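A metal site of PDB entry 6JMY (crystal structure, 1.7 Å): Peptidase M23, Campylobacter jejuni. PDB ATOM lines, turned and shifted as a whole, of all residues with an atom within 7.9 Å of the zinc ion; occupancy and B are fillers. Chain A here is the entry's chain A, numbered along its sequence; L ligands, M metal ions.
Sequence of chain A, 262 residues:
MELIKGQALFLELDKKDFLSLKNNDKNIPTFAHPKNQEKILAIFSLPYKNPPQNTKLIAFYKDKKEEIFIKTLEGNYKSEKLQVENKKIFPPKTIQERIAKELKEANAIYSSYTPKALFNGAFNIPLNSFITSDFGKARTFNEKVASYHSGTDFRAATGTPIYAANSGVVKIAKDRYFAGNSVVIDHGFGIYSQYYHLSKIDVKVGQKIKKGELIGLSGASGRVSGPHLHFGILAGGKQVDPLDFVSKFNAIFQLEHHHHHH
The zinc ion is bound by the side-chain carboxylate (OD1) of Asp 153 (2.0 Å). The zinc ion is bound by ND1 of His 230. The zinc ion is bound by O6 of the ligand, at 2.0 Å. NE2 of His 149 binds the zinc ion, 2.1 Å away. An oxygen (O7) of the ligand is bound to the zinc ion. The zinc ion has five donor atoms within binding distance.
Within 4 Å of the zinc ion: His 149, Asp 153 and His 230.
A ring nitrogen (ND1) of His 149 is in hydrogen-bond range of the backbone carbonyl oxygen (O) of Asp 134 (2.8 Å). The backbone NH (N) of Asp 153 lies within hydrogen-bond range of the backbone carbonyl oxygen (O) of Ser 133 (2.8 Å). The backbone carbonyl oxygen (O) of His 230 sits at hydrogen-bond distance from the backbone NH (N) of Tyr 196 (3.0 Å). ND1 of His 149 lies close to O of Ser 133 (3.3 Å). The backbone NH (N) of Thr 132 is in hydrogen-bond range of the backbone carbonyl oxygen (O) of Asp 153 (2.9 Å). NH2 of Arg 139 lies within salt-bridge range of OD2 of Asp 153 (3.1 Å). A ring nitrogen (ND1) of His 149 lies close to the backbone carbonyl oxygen of Gly 151, at 3.1 Å. NH2 of Arg 139 lies within hydrogen-bond range of ND1 of His 149.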
ATOM      1  N   GLU A  80      16.382   9.248   6.828  1.00  0.00           N
ATOM      2  CA  GLU A  80      15.632   9.112   5.581  1.00  0.00           C
ATOM      3  C   GLU A  80      16.490   9.602   4.421  1.00  0.00           C
ATOM      4  O   GLU A  80      17.398  10.424   4.605  1.00  0.00           O
ATOM      5  CB  GLU A  80      14.298   9.873   5.646  1.00  0.00           C
ATOM      6  CG  GLU A  80      14.366  11.333   5.248  1.00  0.00           C
ATOM      7  CD  GLU A  80      13.017  12.046   5.352  1.00  0.00           C
ATOM      8  OE1 GLU A  80      11.973  11.372   5.469  1.00  0.00           O
ATOM      9  OE2 GLU A  80      13.014  13.292   5.302  1.00  0.00           O
ATOM     10  N   LEU A  82      16.486  11.227   0.453  1.00  0.00           N
ATOM     11  CA  LEU A  82      15.691  12.047  -0.447  1.00  0.00           C
ATOM     12  C   LEU A  82      16.483  12.341  -1.709  1.00  0.00           C
ATOM     13  O   LEU A  82      17.701  12.535  -1.658  1.00  0.00           O
ATOM     14  CB  LEU A  82      15.270  13.360   0.220  1.00  0.00           C
ATOM     15  CG  LEU A  82      14.242  13.241   1.341  1.00  0.00           C
ATOM     16  CD1 LEU A  82      14.006  14.589   1.989  1.00  0.00           C
ATOM     17  CD2 LEU A  82      12.946  12.669   0.776  1.00  0.00           C
ATOM     18  N   THR A 132       3.999  13.224   6.101  1.00  0.00           N
ATOM     19  CA  THR A 132       4.801  12.411   5.201  1.00  0.00           C
ATOM     20  C   THR A 132       6.286  12.403   5.572  1.00  0.00           C
ATOM     21  O   THR A 132       7.002  11.477   5.191  1.00  0.00           O
ATOM     22  CB  THR A 132       4.675  12.916   3.754  1.00  0.00           C
ATOM     23  OG1 THR A 132       4.960  14.310   3.706  1.00  0.00           O
ATOM     24  CG2 THR A 132       3.248  12.694   3.241  1.00  0.00           C
ATOM     25  N   SER A 133       6.749  13.419   6.294  1.00  0.00           N
ATOM     26  CA  SER A 133       8.126  13.455   6.755  1.00  0.00           C
ATOM     27  C   SER A 133       8.138  14.266   8.041  1.00  0.00           C
ATOM     28  O   SER A 133       7.900  15.477   8.028  1.00  0.00           O
ATOM     29  CB  SER A 133       9.047  14.078   5.717  1.00  0.00           C
ATOM     30  OG  SER A 133      10.382  14.071   6.197  1.00  0.00           O
ATOM     31  N   ASP A 134       8.385  13.565   9.158  1.00  0.00           N
ATOM     32  CA  ASP A 134       8.298  14.155  10.482  1.00  0.00           C
ATOM     33  C   ASP A 134       9.505  15.057  10.768  1.00  0.00           C
ATOM     34  O   ASP A 134      10.534  15.016  10.076  1.00  0.00           O
ATOM     35  CB  ASP A 134       8.196  13.052  11.533  1.00  0.00           C
ATOM     36  CG  ASP A 134       7.202  13.378  12.637  1.00  0.00           C
ATOM     37  OD1 ASP A 134       6.917  14.581  12.854  1.00  0.00           O
ATOM     38  OD2 ASP A 134       6.705  12.434  13.276  1.00  0.00           O
ATOM     39  N   PHE A 135       9.366  15.857  11.823  1.00  0.00           N
ATOM     40  CA  PHE A 135      10.442  16.751  12.228  1.00  0.00           C
ATOM     41  C   PHE A 135      11.661  15.968  12.692  1.00  0.00           C
ATOM     42  O   PHE A 135      11.535  14.923  13.343  1.00  0.00           O
ATOM     43  CB  PHE A 135       9.954  17.656  13.361  1.00  0.00           C
ATOM     44  CG  PHE A 135      11.041  18.532  13.936  1.00  0.00           C
ATOM     45  CD1 PHE A 135      11.305  19.776  13.387  1.00  0.00           C
ATOM     46  CD2 PHE A 135      11.776  18.113  15.039  1.00  0.00           C
ATOM     47  CE1 PHE A 135      12.297  20.596  13.921  1.00  0.00           C
ATOM     48  CE2 PHE A 135      12.760  18.927  15.572  1.00  0.00           C
ATOM     49  CZ  PHE A 135      13.030  20.163  15.024  1.00  0.00           C
ATOM     50  N   ARG A 139      18.620  13.386   7.416  1.00  0.00           N
ATOM     51  CA  ARG A 139      18.429  13.249   5.984  1.00  0.00           C
ATOM     52  C   ARG A 139      19.753  13.126   5.253  1.00  0.00           C
ATOM     53  O   ARG A 139      20.786  13.617   5.715  1.00  0.00           O
ATOM     54  CB  ARG A 139      17.640  14.445   5.437  1.00  0.00           C
ATOM     55  CG  ARG A 139      16.199  14.446   5.865  1.00  0.00           C
ATOM     56  CD  ARG A 139      15.510  15.739   5.520  1.00  0.00           C
ATOM     57  NE  ARG A 139      14.072  15.559   5.397  1.00  0.00           N
ATOM     58  CZ  ARG A 139      13.245  16.516   4.988  1.00  0.00           C
ATOM     59  NH1 ARG A 139      13.731  17.723   4.680  1.00  0.00           N
ATOM     60  NH2 ARG A 139      11.946  16.263   4.876  1.00  0.00           N
ATOM     61  N   TYR A 148      19.150  17.740   8.223  1.00  0.00           N
ATOM     62  CA  TYR A 148      18.111  17.316   9.142  1.00  0.00           C
ATOM     63  C   TYR A 148      16.840  18.049   8.777  1.00  0.00           C
ATOM     64  O   TYR A 148      16.874  19.151   8.236  1.00  0.00           O
ATOM     65  CB  TYR A 148      18.485  17.574  10.627  1.00  0.00           C
ATOM     66  CG  TYR A 148      18.051  18.926  11.164  1.00  0.00           C
ATOM     67  CD1 TYR A 148      18.819  20.067  10.938  1.00  0.00           C
ATOM     68  CD2 TYR A 148      16.892  19.059  11.926  1.00  0.00           C
ATOM     69  CE1 TYR A 148      18.417  21.307  11.444  1.00  0.00           C
ATOM     70  CE2 TYR A 148      16.504  20.297  12.432  1.00  0.00           C
ATOM     71  CZ  TYR A 148      17.268  21.410  12.176  1.00  0.00           C
ATOM     72  OH  TYR A 148      16.878  22.634  12.682  1.00  0.00           O
ATOM     73  N   HIS A 149      15.697  17.439   9.084  1.00  0.00           N
ATOM     74  CA  HIS A 149      14.422  18.058   8.759  1.00  0.00           C
ATOM     75  C   HIS A 149      14.033  19.084   9.813  1.00  0.00           C
ATOM     76  O   HIS A 149      13.747  18.725  10.958  1.00  0.00           O
ATOM     77  CB  HIS A 149      13.326  17.001   8.632  1.00  0.00           C
ATOM     78  CG  HIS A 149      12.108  17.514   7.946  1.00  0.00           C
ATOM     79  ND1 HIS A 149      10.900  16.845   7.962  1.00  0.00           N
ATOM     80  CD2 HIS A 149      11.910  18.632   7.203  1.00  0.00           C
ATOM     81  CE1 HIS A 149      10.011  17.535   7.270  1.00  0.00           C
ATOM     82  NE2 HIS A 149      10.601  18.620   6.793  1.00  0.00           N
ATOM     83  N   SER A 150      13.972  20.364   9.422  1.00  0.00           N
ATOM     84  CA  SER A 150      13.712  21.435  10.388  1.00  0.00           C
ATOM     85  C   SER A 150      12.241  21.823  10.500  1.00  0.00           C
ATOM     86  O   SER A 150      11.930  22.833  11.145  1.00  0.00           O
ATOM     87  CB  SER A 150      14.553  22.665  10.054  1.00  0.00           C
ATOM     88  OG  SER A 150      14.178  23.186   8.785  1.00  0.00           O
ATOM     89  N   GLY A 151      11.336  21.054   9.907  1.00  0.00           N
ATOM     90  CA  GLY A 151       9.911  21.242  10.087  1.00  0.00           C
ATOM     91  C   GLY A 151       9.212  19.929   9.872  1.00  0.00           C
ATOM     92  O   GLY A 151       9.846  18.869   9.999  1.00  0.00           O
ATOM     93  N   THR A 152       7.908  19.958   9.562  1.00  0.00           N
ATOM     94  CA  THR A 152       7.153  18.741   9.317  1.00  0.00           C
ATOM     95  C   THR A 152       6.457  18.855   7.962  1.00  0.00           C
ATOM     96  O   THR A 152       5.911  19.918   7.616  1.00  0.00           O
ATOM     97  CB  THR A 152       6.144  18.474  10.467  1.00  0.00           C
ATOM     98  OG1 THR A 152       5.509  17.209  10.273  1.00  0.00           O
ATOM     99  CG2 THR A 152       5.093  19.577  10.557  1.00  0.00           C
ATOM    100  N   ASP A 153       6.524  17.792   7.165  1.00  0.00           N
ATOM    101  CA  ASP A 153       5.918  17.799   5.840  1.00  0.00           C
ATOM    102  C   ASP A 153       4.569  17.102   5.864  1.00  0.00           C
ATOM    103  O   ASP A 153       4.431  16.023   6.455  1.00  0.00           O
ATOM    104  CB  ASP A 153       6.828  17.127   4.812  1.00  0.00           C
ATOM    105  CG  ASP A 153       8.123  17.884   4.608  1.00  0.00           C
ATOM    106  OD1 ASP A 153       8.154  19.093   4.947  1.00  0.00           O
ATOM    107  OD2 ASP A 153       9.099  17.248   4.151  1.00  0.00           O
ATOM    108  N   PHE A 154       3.591  17.727   5.211  1.00  0.00           N
ATOM    109  CA  PHE A 154       2.246  17.181   5.067  1.00  0.00           C
ATOM    110  C   PHE A 154       1.984  16.820   3.612  1.00  0.00           C
ATOM    111  O   PHE A 154       2.420  17.547   2.700  1.00  0.00           O
ATOM    112  CB  PHE A 154       1.187  18.203   5.516  1.00  0.00           C
ATOM    113  CG  PHE A 154       1.143  18.441   6.997  1.00  0.00           C
ATOM    114  CD1 PHE A 154       2.057  19.265   7.611  1.00  0.00           C
ATOM    115  CD2 PHE A 154       0.137  17.855   7.765  1.00  0.00           C
ATOM    116  CE1 PHE A 154       2.003  19.483   8.982  1.00  0.00           C
ATOM    117  CE2 PHE A 154       0.070  18.076   9.126  1.00  0.00           C
ATOM    118  CZ  PHE A 154       1.011  18.896   9.740  1.00  0.00           C
ATOM    119  N   TYR A 196       6.235  26.567   3.468  1.00  0.00           N
ATOM    120  CA  TYR A 196       7.209  26.573   2.385  1.00  0.00           C
ATOM    121  C   TYR A 196       6.748  25.733   1.205  1.00  0.00           C
ATOM    122  O   TYR A 196       5.867  24.869   1.312  1.00  0.00           O
ATOM    123  CB  TYR A 196       8.584  26.052   2.842  1.00  0.00           C
ATOM    124  CG  TYR A 196       9.300  26.868   3.904  1.00  0.00           C
ATOM    125  CD1 TYR A 196       8.933  28.183   4.171  1.00  0.00           C
ATOM    126  CD2 TYR A 196      10.330  26.305   4.638  1.00  0.00           C
ATOM    127  CE1 TYR A 196       9.602  28.928   5.172  1.00  0.00           C
ATOM    128  CE2 TYR A 196      10.998  27.037   5.609  1.00  0.00           C
ATOM    129  CZ  TYR A 196      10.628  28.338   5.875  1.00  0.00           C
ATOM    130  OH  TYR A 196      11.293  29.055   6.846  1.00  0.00           O
ATOM    131  N   HIS A 197       7.413  25.996   0.072  1.00  0.00           N
ATOM    132  CA  HIS A 197       7.284  25.261  -1.194  1.00  0.00           C
ATOM    133  C   HIS A 197       5.949  25.528  -1.873  1.00  0.00           C
ATOM    134  O   HIS A 197       5.530  24.742  -2.722  1.00  0.00           O
ATOM    135  CB  HIS A 197       7.497  23.759  -1.004  1.00  0.00           C
ATOM    136  CG  HIS A 197       8.750  23.433  -0.256  1.00  0.00           C
ATOM    137  ND1 HIS A 197       9.994  23.856  -0.683  1.00  0.00           N
ATOM    138  CD2 HIS A 197       8.952  22.761   0.890  1.00  0.00           C
ATOM    139  CE1 HIS A 197      10.906  23.455   0.181  1.00  0.00           C
ATOM    140  NE2 HIS A 197      10.298  22.776   1.141  1.00  0.00           N
ATOM    141  N   ARG A 223      13.696  23.586  -2.927  1.00  0.00           N
ATOM    142  CA  ARG A 223      14.326  22.276  -2.821  1.00  0.00           C
ATOM    143  C   ARG A 223      13.276  21.264  -2.397  1.00  0.00           C
ATOM    144  O   ARG A 223      12.828  21.281  -1.240  1.00  0.00           O
ATOM    145  CB  ARG A 223      15.497  22.298  -1.832  1.00  0.00           C
ATOM    146  CG  ARG A 223      16.055  20.897  -1.558  1.00  0.00           C
ATOM    147  CD  ARG A 223      17.451  20.923  -0.957  1.00  0.00           C
ATOM    148  NE  ARG A 223      17.428  21.423   0.407  1.00  0.00           N
ATOM    149  CZ  ARG A 223      18.419  22.106   0.970  1.00  0.00           C
ATOM    150  NH1 ARG A 223      19.527  22.382   0.290  1.00  0.00           N
ATOM    151  NH2 ARG A 223      18.298  22.523   2.222  1.00  0.00           N
ATOM    152  N   HIS A 228       4.462  19.003  -1.763  1.00  0.00           N
ATOM    153  CA  HIS A 228       4.022  18.817  -0.378  1.00  0.00           C
ATOM    154  C   HIS A 228       3.989  20.177   0.282  1.00  0.00           C
ATOM    155  O   HIS A 228       4.430  21.179  -0.287  1.00  0.00           O
ATOM    156  CB  HIS A 228       4.933  17.858   0.392  1.00  0.00           C
ATOM    157  CG  HIS A 228       6.337  18.373   0.567  1.00  0.00           C
ATOM    158  ND1 HIS A 228       7.275  18.291  -0.436  1.00  0.00           N
ATOM    159  CD2 HIS A 228       6.932  19.014   1.597  1.00  0.00           C
ATOM    160  CE1 HIS A 228       8.407  18.853  -0.023  1.00  0.00           C
ATOM    161  NE2 HIS A 228       8.225  19.301   1.209  1.00  0.00           N
ATOM    162  N   LEU A 229       3.486  20.217   1.519  1.00  0.00           N
ATOM    163  CA  LEU A 229       3.574  21.405   2.358  1.00  0.00           C
ATOM    164  C   LEU A 229       4.608  21.154   3.445  1.00  0.00           C
ATOM    165  O   LEU A 229       4.588  20.099   4.097  1.00  0.00           O
ATOM    166  CB  LEU A 229       2.233  21.776   3.001  1.00  0.00           C
ATOM    167  CG  LEU A 229       2.398  22.871   4.070  1.00  0.00           C
ATOM    168  CD1 LEU A 229       2.515  24.269   3.431  1.00  0.00           C
ATOM    169  CD2 LEU A 229       1.289  22.829   5.111  1.00  0.00           C
ATOM    170  N   HIS A 230       5.521  22.090   3.619  1.00  0.00           N
ATOM    171  CA  HIS A 230       6.424  22.102   4.746  1.00  0.00           C
ATOM    172  C   HIS A 230       5.932  23.152   5.740  1.00  0.00           C
ATOM    173  O   HIS A 230       5.790  24.323   5.368  1.00  0.00           O
ATOM    174  CB  HIS A 230       7.845  22.419   4.279  1.00  0.00           C
ATOM    175  CG  HIS A 230       8.814  22.665   5.389  1.00  0.00           C
ATOM    176  ND1 HIS A 230       9.743  21.721   5.779  1.00  0.00           N
ATOM    177  CD2 HIS A 230       9.024  23.756   6.169  1.00  0.00           C
ATOM    178  CE1 HIS A 230      10.473  22.213   6.769  1.00  0.00           C
ATOM    179  NE2 HIS A 230      10.065  23.449   7.015  1.00  0.00           N
ATOM    180  N   PHE A 231       5.684  22.722   6.975  1.00  0.00           N
ATOM    181  CA  PHE A 231       5.234  23.592   8.068  1.00  0.00           C
ATOM    182  C   PHE A 231       6.337  23.639   9.117  1.00  0.00           C
ATOM    183  O   PHE A 231       6.879  22.598   9.493  1.00  0.00           O
ATOM    184  CB  PHE A 231       3.916  23.065   8.674  1.00  0.00           C
ATOM    185  CG  PHE A 231       3.395  23.895   9.826  1.00  0.00           C
ATOM    186  CD1 PHE A 231       2.979  25.201   9.622  1.00  0.00           C
ATOM    187  CD2 PHE A 231       3.299  23.341  11.091  1.00  0.00           C
ATOM    188  CE1 PHE A 231       2.496  25.948  10.684  1.00  0.00           C
ATOM    189  CE2 PHE A 231       2.805  24.068  12.153  1.00  0.00           C
ATOM    190  CZ  PHE A 231       2.412  25.378  11.949  1.00  0.00           C
ATOM    191  N   GLY A 232       6.675  24.849   9.559  1.00  0.00           N
ATOM    192  CA  GLY A 232       7.704  25.014  10.558  1.00  0.00           C
ATOM    193  C   GLY A 232       7.283  25.980  11.652  1.00  0.00           C
ATOM    194  O   GLY A 232       6.390  26.802  11.461  1.00  0.00           O
HETATM  195  C1  LIG L   1      13.610  21.066   1.904  1.00  0.00           C
HETATM  196  O1  LIG L   1      12.698  21.873   2.183  1.00  0.00           O
HETATM  197  O2  LIG L   1      14.787  21.490   1.817  1.00  0.00           O
HETATM  198  C2  LIG L   1      13.357  19.584   1.651  1.00  0.00           C
HETATM  199  C3  LIG L   1      11.883  19.179   1.687  1.00  0.00           C
HETATM  200  O3  LIG L   1      11.272  19.751   0.486  1.00  0.00           O
HETATM  201  C4  LIG L   1      11.723  17.665   1.704  1.00  0.00           C
HETATM  202  C5  LIG L   1      11.797  17.078   0.310  1.00  0.00           C
HETATM  203  O4  LIG L   1      10.869  16.354  -0.102  1.00  0.00           O
HETATM  204  O5  LIG L   1      12.782  17.301  -0.420  1.00  0.00           O
HETATM  205  C6  LIG L   1      11.178  19.665   2.945  1.00  0.00           C
HETATM  206  O6  LIG L   1      11.637  19.404   4.067  1.00  0.00           O
HETATM  207  O7  LIG L   1      10.134  20.353   2.862  1.00  0.00           O
HETATM  208 ZN    ZN M   1       9.982  19.805   5.197  1.00  0.00          ZN
